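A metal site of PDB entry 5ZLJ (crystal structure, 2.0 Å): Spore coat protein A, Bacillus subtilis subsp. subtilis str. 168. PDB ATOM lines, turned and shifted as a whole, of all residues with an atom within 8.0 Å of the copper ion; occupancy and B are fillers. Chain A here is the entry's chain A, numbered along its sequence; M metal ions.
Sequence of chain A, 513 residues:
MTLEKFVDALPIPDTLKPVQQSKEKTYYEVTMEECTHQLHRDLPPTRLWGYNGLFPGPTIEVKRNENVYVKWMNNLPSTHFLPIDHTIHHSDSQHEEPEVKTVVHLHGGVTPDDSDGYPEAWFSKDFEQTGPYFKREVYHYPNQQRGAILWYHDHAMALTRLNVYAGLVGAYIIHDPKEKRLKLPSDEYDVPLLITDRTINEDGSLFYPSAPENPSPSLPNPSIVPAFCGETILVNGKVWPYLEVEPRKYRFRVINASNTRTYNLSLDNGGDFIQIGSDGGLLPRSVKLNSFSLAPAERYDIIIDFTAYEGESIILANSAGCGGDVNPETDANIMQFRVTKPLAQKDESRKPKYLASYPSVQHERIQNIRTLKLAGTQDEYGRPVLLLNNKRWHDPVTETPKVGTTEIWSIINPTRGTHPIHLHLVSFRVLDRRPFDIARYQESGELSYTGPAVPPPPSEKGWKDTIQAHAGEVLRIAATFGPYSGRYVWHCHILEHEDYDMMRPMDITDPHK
O of His 497 sits at hydrogen-bond distance from N of Met 502, 2.9 Å away.
A ring nitrogen (NE2) of His 497 sits at hydrogen-bond distance from the backbone carbonyl oxygen (O) of Pro 226, at 3.0 Å.
A ring nitrogen (ND1) of His 419 lies close to the side-chain sulfur (SD) of Met 502.
NE2 of His 419 sits at hydrogen-bond distance from OG1 of Thr 415 (2.9 Å).
The backbone NH of Ala 469 sits at hydrogen-bond distance from the backbone carbonyl oxygen of His 419, at 2.9 Å.
The backbone NH (N) of Cys 492 sits at hydrogen-bond distance from the backbone carbonyl oxygen (O) of Met 502 (3.0 Å).
The backbone NH (N) of Ile 494 sits close to the side-chain sulfur (SG) of Cys 492 (3.4 Å).
The backbone NH (N) of Met 502 is in hydrogen-bond range of the backbone carbonyl oxygen (O) of Leu 386, at 3.0 Å.
Merely in contact with the copper ion: Met 502 (3.2 Å) and Ile 494 (3.98 Å).
The copper ion is bound by a ring nitrogen (ND1) of His 497 (2.1 Å), a ring nitrogen (ND1) of His 419 (2.1 Å) and the side-chain sulfur of Cys 492 (2.2 Å).
The copper ion has three donor atoms within binding distance.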
ATOM      1  N   PRO A 226      22.624  14.473  -5.383  1.00  0.00           N
ATOM      2  CA  PRO A 226      21.715  14.221  -4.252  1.00  0.00           C
ATOM      3  C   PRO A 226      20.636  13.210  -4.540  1.00  0.00           C
ATOM      4  O   PRO A 226      19.844  12.909  -3.651  1.00  0.00           O
ATOM      5  CB  PRO A 226      21.068  15.585  -3.998  1.00  0.00           C
ATOM      6  CG  PRO A 226      21.147  16.289  -5.317  1.00  0.00           C
ATOM      7  CD  PRO A 226      22.367  15.789  -6.018  1.00  0.00           C
ATOM      8  N   LEU A 374      14.876  15.947  10.174  1.00  0.00           N
ATOM      9  CA  LEU A 374      15.530  15.706   8.918  1.00  0.00           C
ATOM     10  C   LEU A 374      15.830  17.056   8.285  1.00  0.00           C
ATOM     11  O   LEU A 374      14.939  17.820   7.997  1.00  0.00           O
ATOM     12  CB  LEU A 374      14.627  14.901   7.984  1.00  0.00           C
ATOM     13  CG  LEU A 374      14.047  13.603   8.594  1.00  0.00           C
ATOM     14  CD1 LEU A 374      13.266  12.822   7.523  1.00  0.00           C
ATOM     15  CD2 LEU A 374      15.119  12.754   9.240  1.00  0.00           C
ATOM     16  N   ALA A 375      17.101  17.325   8.063  1.00  0.00           N
ATOM     17  CA  ALA A 375      17.514  18.640   7.587  1.00  0.00           C
ATOM     18  C   ALA A 375      18.796  18.542   6.743  1.00  0.00           C
ATOM     19  O   ALA A 375      19.006  17.572   6.030  1.00  0.00           O
ATOM     20  CB  ALA A 375      17.699  19.583   8.782  1.00  0.00           C
ATOM     21  N   LEU A 386      22.789  16.514   3.384  1.00  0.00           N
ATOM     22  CA  LEU A 386      21.606  16.112   4.119  1.00  0.00           C
ATOM     23  C   LEU A 386      22.011  15.521   5.476  1.00  0.00           C
ATOM     24  O   LEU A 386      22.898  14.661   5.537  1.00  0.00           O
ATOM     25  CB  LEU A 386      20.792  15.123   3.299  1.00  0.00           C
ATOM     26  CG  LEU A 386      20.256  15.833   2.056  1.00  0.00           C
ATOM     27  CD1 LEU A 386      20.856  15.336   0.754  1.00  0.00           C
ATOM     28  CD2 LEU A 386      18.748  15.796   2.062  1.00  0.00           C
ATOM     29  N   LEU A 387      21.354  15.962   6.543  1.00  0.00           N
ATOM     30  CA  LEU A 387      21.739  15.648   7.919  1.00  0.00           C
ATOM     31  C   LEU A 387      20.571  15.221   8.771  1.00  0.00           C
ATOM     32  O   LEU A 387      19.446  15.694   8.616  1.00  0.00           O
ATOM     33  CB  LEU A 387      22.390  16.878   8.574  1.00  0.00           C
ATOM     34  CG  LEU A 387      23.611  17.468   7.889  1.00  0.00           C
ATOM     35  CD1 LEU A 387      24.122  18.684   8.686  1.00  0.00           C
ATOM     36  CD2 LEU A 387      24.686  16.436   7.718  1.00  0.00           C
ATOM     37  N   LEU A 388      20.865  14.317   9.719  1.00  0.00           N
ATOM     38  CA  LEU A 388      19.881  13.906  10.693  1.00  0.00           C
ATOM     39  C   LEU A 388      20.158  14.738  11.980  1.00  0.00           C
ATOM     40  O   LEU A 388      21.277  14.720  12.521  1.00  0.00           O
ATOM     41  CB  LEU A 388      20.028  12.422  10.977  1.00  0.00           C
ATOM     42  CG  LEU A 388      19.852  11.480   9.771  1.00  0.00           C
ATOM     43  CD1 LEU A 388      20.263  10.093  10.172  1.00  0.00           C
ATOM     44  CD2 LEU A 388      18.432  11.503   9.274  1.00  0.00           C
ATOM     45  N   ASN A 413       9.956  15.934   9.392  1.00  0.00           N
ATOM     46  CA  ASN A 413      10.458  16.160   8.062  1.00  0.00           C
ATOM     47  C   ASN A 413       9.959  17.479   7.481  1.00  0.00           C
ATOM     48  O   ASN A 413       8.867  17.502   6.889  1.00  0.00           O
ATOM     49  CB  ASN A 413      10.013  15.043   7.097  1.00  0.00           C
ATOM     50  CG  ASN A 413      10.659  15.204   5.734  1.00  0.00           C
ATOM     51  OD1 ASN A 413      11.417  16.142   5.491  1.00  0.00           O
ATOM     52  ND2 ASN A 413      10.353  14.288   4.838  1.00  0.00           N
ATOM     53  N   THR A 415      11.539  18.956   4.982  1.00  0.00           N
ATOM     54  CA  THR A 415      12.133  19.079   3.644  1.00  0.00           C
ATOM     55  C   THR A 415      11.041  18.913   2.623  1.00  0.00           C
ATOM     56  O   THR A 415       9.901  18.655   2.969  1.00  0.00           O
ATOM     57  CB  THR A 415      13.277  18.031   3.361  1.00  0.00           C
ATOM     58  OG1 THR A 415      12.720  16.699   3.174  1.00  0.00           O
ATOM     59  CG2 THR A 415      14.349  18.042   4.478  1.00  0.00           C
ATOM     60  N   GLY A 417      10.885  16.500   0.311  1.00  0.00           N
ATOM     61  CA  GLY A 417      10.651  15.138  -0.198  1.00  0.00           C
ATOM     62  C   GLY A 417      10.548  14.104   0.897  1.00  0.00           C
ATOM     63  O   GLY A 417      10.799  14.397   2.079  1.00  0.00           O
ATOM     64  N   THR A 418      10.158  12.899   0.507  1.00  0.00           N
ATOM     65  CA  THR A 418      10.115  11.761   1.396  1.00  0.00           C
ATOM     66  C   THR A 418      11.502  11.176   1.643  1.00  0.00           C
ATOM     67  O   THR A 418      12.322  11.157   0.735  1.00  0.00           O
ATOM     68  CB  THR A 418       9.194  10.672   0.794  1.00  0.00           C
ATOM     69  OG1 THR A 418       7.868  11.183   0.731  1.00  0.00           O
ATOM     70  CG2 THR A 418       9.144   9.417   1.641  1.00  0.00           C
ATOM     71  N   HIS A 419      11.797  10.771   2.896  1.00  0.00           N
ATOM     72  CA  HIS A 419      13.023  10.052   3.212  1.00  0.00           C
ATOM     73  C   HIS A 419      12.680   8.701   3.802  1.00  0.00           C
ATOM     74  O   HIS A 419      11.944   8.650   4.783  1.00  0.00           O
ATOM     75  CB  HIS A 419      13.887  10.843   4.195  1.00  0.00           C
ATOM     76  CG  HIS A 419      14.267  12.187   3.688  1.00  0.00           C
ATOM     77  ND1 HIS A 419      15.344  12.372   2.880  1.00  0.00           N
ATOM     78  CD2 HIS A 419      13.675  13.403   3.818  1.00  0.00           C
ATOM     79  CE1 HIS A 419      15.445  13.654   2.552  1.00  0.00           C
ATOM     80  NE2 HIS A 419      14.417  14.293   3.081  1.00  0.00           N
ATOM     81  N   PRO A 420      13.190   7.605   3.217  1.00  0.00           N
ATOM     82  CA  PRO A 420      12.951   6.296   3.814  1.00  0.00           C
ATOM     83  C   PRO A 420      13.969   6.036   4.919  1.00  0.00           C
ATOM     84  O   PRO A 420      15.133   5.801   4.633  1.00  0.00           O
ATOM     85  CB  PRO A 420      13.142   5.321   2.648  1.00  0.00           C
ATOM     86  CG  PRO A 420      14.144   6.003   1.776  1.00  0.00           C
ATOM     87  CD  PRO A 420      13.958   7.502   1.964  1.00  0.00           C
ATOM     88  N   ILE A 421      13.542   6.150   6.171  1.00  0.00           N
ATOM     89  CA  ILE A 421      14.419   6.013   7.320  1.00  0.00           C
ATOM     90  C   ILE A 421      14.521   4.557   7.764  1.00  0.00           C
ATOM     91  O   ILE A 421      13.508   3.899   7.976  1.00  0.00           O
ATOM     92  CB  ILE A 421      13.927   6.892   8.476  1.00  0.00           C
ATOM     93  CG1 ILE A 421      13.776   8.353   8.012  1.00  0.00           C
ATOM     94  CG2 ILE A 421      14.873   6.726   9.693  1.00  0.00           C
ATOM     95  CD1 ILE A 421      15.052   8.983   7.504  1.00  0.00           C
ATOM     96  N   ALA A 469       9.150   8.682   5.662  1.00  0.00           N
ATOM     97  CA  ALA A 469       8.877   9.914   6.402  1.00  0.00           C
ATOM     98  C   ALA A 469       8.591  10.956   5.346  1.00  0.00           C
ATOM     99  O   ALA A 469       9.513  11.464   4.693  1.00  0.00           O
ATOM    100  CB  ALA A 469      10.075  10.295   7.258  1.00  0.00           C
ATOM    101  N   HIS A 491      19.681   5.739   9.474  1.00  0.00           N
ATOM    102  CA  HIS A 491      19.961   6.556   8.314  1.00  0.00           C
ATOM    103  C   HIS A 491      18.835   6.600   7.299  1.00  0.00           C
ATOM    104  O   HIS A 491      17.904   5.749   7.300  1.00  0.00           O
ATOM    105  CB  HIS A 491      21.240   6.075   7.617  1.00  0.00           C
ATOM    106  CG  HIS A 491      21.153   4.678   7.066  1.00  0.00           C
ATOM    107  ND1 HIS A 491      20.945   4.415   5.731  1.00  0.00           N
ATOM    108  CD2 HIS A 491      21.323   3.474   7.667  1.00  0.00           C
ATOM    109  CE1 HIS A 491      20.936   3.114   5.539  1.00  0.00           C
ATOM    110  NE2 HIS A 491      21.183   2.526   6.689  1.00  0.00           N
ATOM    111  N   CYS A 492      18.929   7.582   6.417  1.00  0.00           N
ATOM    112  CA  CYS A 492      18.090   7.625   5.229  1.00  0.00           C
ATOM    113  C   CYS A 492      18.639   6.592   4.248  1.00  0.00           C
ATOM    114  O   CYS A 492      19.861   6.463   4.089  1.00  0.00           O
ATOM    115  CB  CYS A 492      18.089   9.015   4.600  1.00  0.00           C
ATOM    116  SG  CYS A 492      17.169   9.019   3.059  1.00  0.00           S
ATOM    117  N   HIS A 493      17.736   5.860   3.599  1.00  0.00           N
ATOM    118  CA  HIS A 493      18.154   4.823   2.667  1.00  0.00           C
ATOM    119  C   HIS A 493      18.120   5.236   1.222  1.00  0.00           C
ATOM    120  O   HIS A 493      18.229   4.397   0.313  1.00  0.00           O
ATOM    121  CB  HIS A 493      17.368   3.511   2.893  1.00  0.00           C
ATOM    122  CG  HIS A 493      18.239   2.294   2.712  1.00  0.00           C
ATOM    123  ND1 HIS A 493      18.679   1.888   1.470  1.00  0.00           N
ATOM    124  CD2 HIS A 493      18.746   1.411   3.605  1.00  0.00           C
ATOM    125  CE1 HIS A 493      19.450   0.810   1.614  1.00  0.00           C
ATOM    126  NE2 HIS A 493      19.501   0.507   2.899  1.00  0.00           N
ATOM    127  N   ILE A 494      17.961   6.531   0.952  1.00  0.00           N
ATOM    128  CA  ILE A 494      18.356   7.045  -0.337  1.00  0.00           C
ATOM    129  C   ILE A 494      19.877   7.157  -0.266  1.00  0.00           C
ATOM    130  O   ILE A 494      20.428   7.920   0.564  1.00  0.00           O
ATOM    131  CB  ILE A 494      17.698   8.405  -0.656  1.00  0.00           C
ATOM    132  CG1 ILE A 494      16.189   8.201  -0.813  1.00  0.00           C
ATOM    133  CG2 ILE A 494      18.324   9.039  -1.888  1.00  0.00           C
ATOM    134  CD1 ILE A 494      15.368   9.464  -0.831  1.00  0.00           C
ATOM    135  N   LEU A 495      20.558   6.368  -1.086  1.00  0.00           N
ATOM    136  CA  LEU A 495      21.987   6.145  -0.868  1.00  0.00           C
ATOM    137  C   LEU A 495      22.791   7.417  -1.122  1.00  0.00           C
ATOM    138  O   LEU A 495      23.760   7.694  -0.409  1.00  0.00           O
ATOM    139  CB  LEU A 495      22.514   4.986  -1.695  1.00  0.00           C
ATOM    140  CG  LEU A 495      21.799   3.667  -1.442  1.00  0.00           C
ATOM    141  CD1 LEU A 495      22.468   2.536  -2.242  1.00  0.00           C
ATOM    142  CD2 LEU A 495      21.746   3.315   0.044  1.00  0.00           C
ATOM    143  N   GLU A 496      22.335   8.216  -2.087  1.00  0.00           N
ATOM    144  CA  GLU A 496      22.915   9.529  -2.367  1.00  0.00           C
ATOM    145  C   GLU A 496      22.831  10.497  -1.154  1.00  0.00           C
ATOM    146  O   GLU A 496      23.681  11.383  -0.987  1.00  0.00           O
ATOM    147  CB  GLU A 496      22.259  10.150  -3.602  1.00  0.00           C
ATOM    148  CG  GLU A 496      22.664   9.556  -4.946  1.00  0.00           C
ATOM    149  CD  GLU A 496      22.229   8.111  -5.191  1.00  0.00           C
ATOM    150  OE1 GLU A 496      21.201   7.675  -4.602  1.00  0.00           O
ATOM    151  OE2 GLU A 496      22.947   7.416  -5.967  1.00  0.00           O
ATOM    152  N   HIS A 497      21.796  10.328  -0.320  1.00  0.00           N
ATOM    153  CA  HIS A 497      21.679  11.095   0.918  1.00  0.00           C
ATOM    154  C   HIS A 497      22.549  10.503   1.998  1.00  0.00           C
ATOM    155  O   HIS A 497      23.240  11.221   2.732  1.00  0.00           O
ATOM    156  CB  HIS A 497      20.242  11.067   1.409  1.00  0.00           C
ATOM    157  CG  HIS A 497      19.299  11.761   0.486  1.00  0.00           C
ATOM    158  ND1 HIS A 497      17.964  11.912   0.777  1.00  0.00           N
ATOM    159  CD2 HIS A 497      19.510  12.369  -0.698  1.00  0.00           C
ATOM    160  CE1 HIS A 497      17.383  12.577  -0.226  1.00  0.00           C
ATOM    161  NE2 HIS A 497      18.294  12.851  -1.125  1.00  0.00           N
ATOM    162  N   GLU A 498      22.452   9.178   2.141  1.00  0.00           N
ATOM    163  CA  GLU A 498      23.194   8.415   3.148  1.00  0.00           C
ATOM    164  C   GLU A 498      24.687   8.759   3.133  1.00  0.00           C
ATOM    165  O   GLU A 498      25.291   8.928   4.203  1.00  0.00           O
ATOM    166  CB  GLU A 498      23.001   6.911   2.896  1.00  0.00           C
ATOM    167  CG  GLU A 498      23.832   6.014   3.780  1.00  0.00           C
ATOM    168  CD  GLU A 498      23.509   4.549   3.549  1.00  0.00           C
ATOM    169  OE1 GLU A 498      22.406   4.231   3.087  1.00  0.00           O
ATOM    170  OE2 GLU A 498      24.330   3.720   3.889  1.00  0.00           O
ATOM    171  N   MET A 502      23.527  11.679   5.561  1.00  0.00           N
ATOM    172  CA  MET A 502      22.282  11.445   6.283  1.00  0.00           C
ATOM    173  C   MET A 502      22.273  10.083   6.981  1.00  0.00           C
ATOM    174  O   MET A 502      21.416   9.231   6.750  1.00  0.00           O
ATOM    175  CB  MET A 502      21.120  11.662   5.348  1.00  0.00           C
ATOM    176  CG  MET A 502      19.805  11.962   6.006  1.00  0.00           C
ATOM    177  SD  MET A 502      18.572  12.474   4.797  1.00  0.00           S
ATOM    178  CE  MET A 502      17.226  12.928   5.837  1.00  0.00           C
HETATM  179 CU    CU M   1      16.967  11.096   2.424  1.00  0.00          CU
